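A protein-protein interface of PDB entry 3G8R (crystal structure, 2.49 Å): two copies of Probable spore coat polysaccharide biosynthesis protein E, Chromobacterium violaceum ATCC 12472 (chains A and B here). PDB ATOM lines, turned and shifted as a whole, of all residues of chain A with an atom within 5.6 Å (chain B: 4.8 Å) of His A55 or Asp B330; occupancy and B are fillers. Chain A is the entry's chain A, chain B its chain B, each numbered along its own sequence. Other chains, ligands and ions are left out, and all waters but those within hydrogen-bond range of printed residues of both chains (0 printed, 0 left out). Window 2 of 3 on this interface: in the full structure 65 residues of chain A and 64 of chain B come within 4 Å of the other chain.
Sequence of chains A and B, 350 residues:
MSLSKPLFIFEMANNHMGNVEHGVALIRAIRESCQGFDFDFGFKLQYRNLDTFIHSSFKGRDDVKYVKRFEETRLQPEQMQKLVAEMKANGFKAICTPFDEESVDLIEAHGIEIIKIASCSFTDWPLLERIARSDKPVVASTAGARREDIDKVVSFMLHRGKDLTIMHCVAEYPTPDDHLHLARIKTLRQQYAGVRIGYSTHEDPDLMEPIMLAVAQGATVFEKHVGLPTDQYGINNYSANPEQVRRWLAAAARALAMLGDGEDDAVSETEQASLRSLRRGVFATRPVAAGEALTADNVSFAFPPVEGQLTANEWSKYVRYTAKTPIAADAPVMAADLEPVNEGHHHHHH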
ATOM      1  N   THR A  52      -3.848   5.954   3.758  1.00  0.00           N
ATOM      2  CA  THR A  52      -3.321   4.835   2.992  1.00  0.00           C
ATOM      3  C   THR A  52      -2.669   3.809   3.921  1.00  0.00           C
ATOM      4  O   THR A  52      -2.749   2.597   3.696  1.00  0.00           O
ATOM      5  CB  THR A  52      -2.248   5.302   1.952  1.00  0.00           C
ATOM      6  OG1 THR A  52      -1.279   6.139   2.592  1.00  0.00           O
ATOM      7  CG2 THR A  52      -2.875   6.083   0.804  1.00  0.00           C
ATOM      8  N   PHE A  53      -2.028   4.308   4.971  1.00  0.00           N
ATOM      9  CA  PHE A  53      -1.077   3.519   5.710  1.00  0.00           C
ATOM     10  C   PHE A  53      -1.711   2.468   6.565  1.00  0.00           C
ATOM     11  O   PHE A  53      -1.188   1.352   6.681  1.00  0.00           O
ATOM     12  CB  PHE A  53      -0.209   4.402   6.594  1.00  0.00           C
ATOM     13  CG  PHE A  53       0.936   3.671   7.204  1.00  0.00           C
ATOM     14  CD1 PHE A  53       0.881   3.266   8.533  1.00  0.00           C
ATOM     15  CD2 PHE A  53       2.038   3.341   6.440  1.00  0.00           C
ATOM     16  CE1 PHE A  53       1.931   2.566   9.114  1.00  0.00           C
ATOM     17  CE2 PHE A  53       3.100   2.648   6.989  1.00  0.00           C
ATOM     18  CZ  PHE A  53       3.055   2.255   8.341  1.00  0.00           C
ATOM     19  N   ILE A  54      -2.806   2.838   7.210  1.00  0.00           N
ATOM     20  CA  ILE A  54      -3.545   1.884   8.009  1.00  0.00           C
ATOM     21  C   ILE A  54      -4.603   1.298   7.114  1.00  0.00           C
ATOM     22  O   ILE A  54      -5.493   1.996   6.623  1.00  0.00           O
ATOM     23  CB  ILE A  54      -4.173   2.520   9.251  1.00  0.00           C
ATOM     24  CG1 ILE A  54      -3.077   3.194  10.099  1.00  0.00           C
ATOM     25  CG2 ILE A  54      -5.014   1.460  10.007  1.00  0.00           C
ATOM     26  CD1 ILE A  54      -3.451   3.497  11.562  1.00  0.00           C
ATOM     27  N   HIS A  55      -4.491   0.008   6.886  1.00  0.00           N
ATOM     28  CA  HIS A  55      -5.360  -0.625   5.940  1.00  0.00           C
ATOM     29  C   HIS A  55      -6.814  -0.669   6.417  1.00  0.00           C
ATOM     30  O   HIS A  55      -7.085  -0.858   7.612  1.00  0.00           O
ATOM     31  CB  HIS A  55      -4.864  -2.018   5.629  1.00  0.00           C
ATOM     32  CG  HIS A  55      -5.568  -2.639   4.475  1.00  0.00           C
ATOM     33  ND1 HIS A  55      -6.569  -3.568   4.634  1.00  0.00           N
ATOM     34  CD2 HIS A  55      -5.458  -2.422   3.146  1.00  0.00           C
ATOM     35  CE1 HIS A  55      -7.021  -3.929   3.451  1.00  0.00           C
ATOM     36  NE2 HIS A  55      -6.363  -3.247   2.531  1.00  0.00           N
ATOM     37  N   SER A  56      -7.742  -0.514   5.475  1.00  0.00           N
ATOM     38  CA  SER A  56      -9.160  -0.648   5.779  1.00  0.00           C
ATOM     39  C   SER A  56      -9.404  -1.737   6.835  1.00  0.00           C
ATOM     40  O   SER A  56     -10.094  -1.484   7.833  1.00  0.00           O
ATOM     41  CB  SER A  56      -9.952  -0.965   4.524  1.00  0.00           C
ATOM     42  OG  SER A  56      -9.504  -0.176   3.434  1.00  0.00           O
ATOM     43  N   SER A  57      -8.815  -2.917   6.607  1.00  0.00           N
ATOM     44  CA  SER A  57      -9.071  -4.108   7.406  1.00  0.00           C
ATOM     45  C   SER A  57      -8.669  -3.922   8.867  1.00  0.00           C
ATOM     46  O   SER A  57      -9.203  -4.574   9.767  1.00  0.00           O
ATOM     47  CB  SER A  57      -8.363  -5.332   6.799  1.00  0.00           C
ATOM     48  OG  SER A  57      -6.950  -5.288   6.990  1.00  0.00           O
ATOM     49  N   PHE A  58      -7.725  -3.021   9.107  1.00  0.00           N
ATOM     50  CA  PHE A  58      -7.289  -2.785  10.467  1.00  0.00           C
ATOM     51  C   PHE A  58      -7.762  -1.484  11.126  1.00  0.00           C
ATOM     52  O   PHE A  58      -7.528  -1.277  12.304  1.00  0.00           O
ATOM     53  CB  PHE A  58      -5.804  -2.986  10.561  1.00  0.00           C
ATOM     54  CG  PHE A  58      -5.426  -4.422  10.692  1.00  0.00           C
ATOM     55  CD1 PHE A  58      -5.286  -5.010  11.959  1.00  0.00           C
ATOM     56  CD2 PHE A  58      -5.231  -5.204   9.564  1.00  0.00           C
ATOM     57  CE1 PHE A  58      -4.938  -6.354  12.094  1.00  0.00           C
ATOM     58  CE2 PHE A  58      -4.880  -6.550   9.680  1.00  0.00           C
ATOM     59  CZ  PHE A  58      -4.737  -7.126  10.951  1.00  0.00           C
ATOM     60  N   LYS A  59      -8.465  -0.634  10.388  1.00  0.00           N
ATOM     61  CA  LYS A  59      -9.044   0.560  10.963  1.00  0.00           C
ATOM     62  C   LYS A  59      -9.838   0.256  12.244  1.00  0.00           C
ATOM     63  O   LYS A  59     -10.578  -0.742  12.319  1.00  0.00           O
ATOM     64  CB  LYS A  59      -9.956   1.228   9.932  1.00  0.00           C
ATOM     65  CG  LYS A  59      -9.449   2.545   9.374  1.00  0.00           C
ATOM     66  CD  LYS A  59      -8.602   2.345   8.147  1.00  0.00           C
ATOM     67  CE  LYS A  59      -8.722   3.548   7.240  1.00  0.00           C
ATOM     68  NZ  LYS A  59      -7.405   3.871   6.654  1.00  0.00           N
ATOM     69  N   PHE B 283      -1.320  -5.878  -0.147  1.00  0.00           N
ATOM     70  CA  PHE B 283      -2.737  -6.102  -0.352  1.00  0.00           C
ATOM     71  C   PHE B 283      -3.045  -5.976  -1.806  1.00  0.00           C
ATOM     72  O   PHE B 283      -2.542  -5.077  -2.472  1.00  0.00           O
ATOM     73  CB  PHE B 283      -3.565  -5.064   0.403  1.00  0.00           C
ATOM     74  CG  PHE B 283      -3.352  -5.080   1.887  1.00  0.00           C
ATOM     75  CD1 PHE B 283      -4.307  -5.657   2.734  1.00  0.00           C
ATOM     76  CD2 PHE B 283      -2.198  -4.518   2.447  1.00  0.00           C
ATOM     77  CE1 PHE B 283      -4.113  -5.672   4.136  1.00  0.00           C
ATOM     78  CE2 PHE B 283      -1.976  -4.543   3.838  1.00  0.00           C
ATOM     79  CZ  PHE B 283      -2.941  -5.116   4.685  1.00  0.00           C
ATOM     80  N   ALA B 284      -3.885  -6.887  -2.279  1.00  0.00           N
ATOM     81  CA  ALA B 284      -4.410  -6.882  -3.630  1.00  0.00           C
ATOM     82  C   ALA B 284      -5.440  -5.767  -3.766  1.00  0.00           C
ATOM     83  O   ALA B 284      -6.367  -5.692  -2.956  1.00  0.00           O
ATOM     84  CB  ALA B 284      -5.045  -8.212  -3.909  1.00  0.00           C
ATOM     85  N   THR B 285      -5.273  -4.901  -4.775  1.00  0.00           N
ATOM     86  CA  THR B 285      -6.213  -3.785  -5.028  1.00  0.00           C
ATOM     87  C   THR B 285      -7.356  -4.085  -6.027  1.00  0.00           C
ATOM     88  O   THR B 285      -8.367  -3.360  -6.071  1.00  0.00           O
ATOM     89  CB  THR B 285      -5.508  -2.448  -5.399  1.00  0.00           C
ATOM     90  OG1 THR B 285      -4.509  -2.665  -6.407  1.00  0.00           O
ATOM     91  CG2 THR B 285      -4.886  -1.787  -4.167  1.00  0.00           C
ATOM     92  N   ALA B 302       0.338  -1.447   2.838  1.00  0.00           N
ATOM     93  CA  ALA B 302      -0.302  -0.855   4.005  1.00  0.00           C
ATOM     94  C   ALA B 302       0.037  -1.653   5.237  1.00  0.00           C
ATOM     95  O   ALA B 302       0.585  -2.742   5.143  1.00  0.00           O
ATOM     96  CB  ALA B 302      -1.797  -0.803   3.820  1.00  0.00           C
ATOM     97  N   PHE B 303      -0.331  -1.138   6.394  1.00  0.00           N
ATOM     98  CA  PHE B 303       0.086  -1.735   7.638  1.00  0.00           C
ATOM     99  C   PHE B 303      -1.128  -2.144   8.462  1.00  0.00           C
ATOM    100  O   PHE B 303      -2.186  -1.582   8.296  1.00  0.00           O
ATOM    101  CB  PHE B 303       1.038  -0.757   8.345  1.00  0.00           C
ATOM    102  CG  PHE B 303       0.786  -0.579   9.814  1.00  0.00           C
ATOM    103  CD1 PHE B 303       1.630  -1.159  10.752  1.00  0.00           C
ATOM    104  CD2 PHE B 303      -0.268   0.211  10.266  1.00  0.00           C
ATOM    105  CE1 PHE B 303       1.421  -0.983  12.129  1.00  0.00           C
ATOM    106  CE2 PHE B 303      -0.500   0.380  11.650  1.00  0.00           C
ATOM    107  CZ  PHE B 303       0.355  -0.213  12.577  1.00  0.00           C
ATOM    108  N   ALA B 328      -8.720 -12.287  -3.698  1.00  0.00           N
ATOM    109  CA  ALA B 328      -9.787 -11.284  -3.721  1.00  0.00           C
ATOM    110  C   ALA B 328      -9.245  -9.854  -3.623  1.00  0.00           C
ATOM    111  O   ALA B 328      -8.243  -9.612  -2.958  1.00  0.00           O
ATOM    112  CB  ALA B 328     -10.782 -11.553  -2.595  1.00  0.00           C
ATOM    113  N   ALA B 329      -9.913  -8.905  -4.271  1.00  0.00           N
ATOM    114  CA  ALA B 329      -9.632  -7.503  -3.998  1.00  0.00           C
ATOM    115  C   ALA B 329      -9.629  -7.264  -2.484  1.00  0.00           C
ATOM    116  O   ALA B 329     -10.363  -7.932  -1.724  1.00  0.00           O
ATOM    117  CB  ALA B 329     -10.641  -6.602  -4.667  1.00  0.00           C
ATOM    118  N   ASP B 330      -8.763  -6.330  -2.072  1.00  0.00           N
ATOM    119  CA  ASP B 330      -8.672  -5.812  -0.697  1.00  0.00           C
ATOM    120  C   ASP B 330      -8.091  -6.815   0.315  1.00  0.00           C
ATOM    121  O   ASP B 330      -7.991  -6.527   1.518  1.00  0.00           O
ATOM    122  CB  ASP B 330     -10.026  -5.217  -0.253  1.00  0.00           C
ATOM    123  CG  ASP B 330     -10.433  -3.980  -1.097  1.00  0.00           C
ATOM    124  OD1 ASP B 330     -11.401  -4.073  -1.905  1.00  0.00           O
ATOM    125  OD2 ASP B 330      -9.760  -2.918  -0.965  1.00  0.00           O
ATOM    126  N   ALA B 331      -7.672  -7.978  -0.190  1.00  0.00           N
ATOM    127  CA  ALA B 331      -7.129  -9.044   0.654  1.00  0.00           C
ATOM    128  C   ALA B 331      -5.580  -9.013   0.780  1.00  0.00           C
ATOM    129  O   ALA B 331      -4.886  -8.466  -0.087  1.00  0.00           O
ATOM    130  CB  ALA B 331      -7.625 -10.409   0.168  1.00  0.00           C
ATOM    131  N   PRO B 332      -5.049  -9.554   1.898  1.00  0.00           N
ATOM    132  CA  PRO B 332      -3.603  -9.720   2.095  1.00  0.00           C
ATOM    133  C   PRO B 332      -3.022 -10.701   1.098  1.00  0.00           C
ATOM    134  O   PRO B 332      -3.582 -11.790   0.906  1.00  0.00           O
ATOM    135  CB  PRO B 332      -3.500 -10.342   3.497  1.00  0.00           C
ATOM    136  CG  PRO B 332      -4.887 -10.838   3.826  1.00  0.00           C
ATOM    137  CD  PRO B 332      -5.804  -9.869   3.125  1.00  0.00           C
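The backbone carbonyl oxygen (O) of Phe A53 sits at hydrogen-bond distance from the backbone NH (N) of Phe B303 (2.6 Å). O of Phe B303 lies within hydrogen-bond range of N of His A55.
The backbone carbonyl oxygen (O) of Ala B284 lies within hydrogen-bond range of the backbone NH (N) of Asp B330, 2.6 Å away. The side-chain amino group (NZ) of Lys A59 sits at hydrogen-bond distance from the backbone carbonyl oxygen (O) of Ile A54 (2.7 Å). A ring nitrogen (ND1) of His A55 is in hydrogen-bond range of the side-chain hydroxyl of Ser A57.
Among the printed residues, merely in contact across the chains: His A55 with Phe B283, His A55 with Asp B330, Thr A52 with Ala B302, Phe A53 with Ala B302, Ile A54 with Phe B303 and His A55 with Ala B302.
Of the printed residues of chain B, His A55 touches Phe B283, Ala B302, Phe B303 and Asp B330. Of the printed residues of chain A, Phe B283 touches His A55 (3.2 Å). Printed residues of chain A within 4 Å of Phe B303: Phe A53 (2.6 Å), Ile A54 (3.7 Å) and His A55 (3.1 Å). Asp B330 touches one residue of chain A. Ala B331 touches none of the printed residues of chain A.
Of the 8 printed residues of chain A, 4 touch a printed residue of chain B. Hydrophobic or aromatic side chains of chain A within 4 Å of the printed part of chain B: Phe A53 and His A55. Of the 10 printed residues of chain B, 4 touch a printed residue of chain A. Hydrophobic or aromatic side chains of chain B within 4 Å of the printed part of chain A: Phe B283, Ala B302 and Phe B303. Along chain B the printed residues that touch a printed residue of chain A span positions 283 to 330. Among the printed residues, 8 pairs touch across the chains. Among the printed residues, no Asp or Glu carboxylate lies within 4 Å of a Lys or Arg side-chain nitrogen of the other chain.
No position is printed for both chains. Of the 8 pairs that touch across the chains among the printed residues, none has its exchanged pair printed and touching as well.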
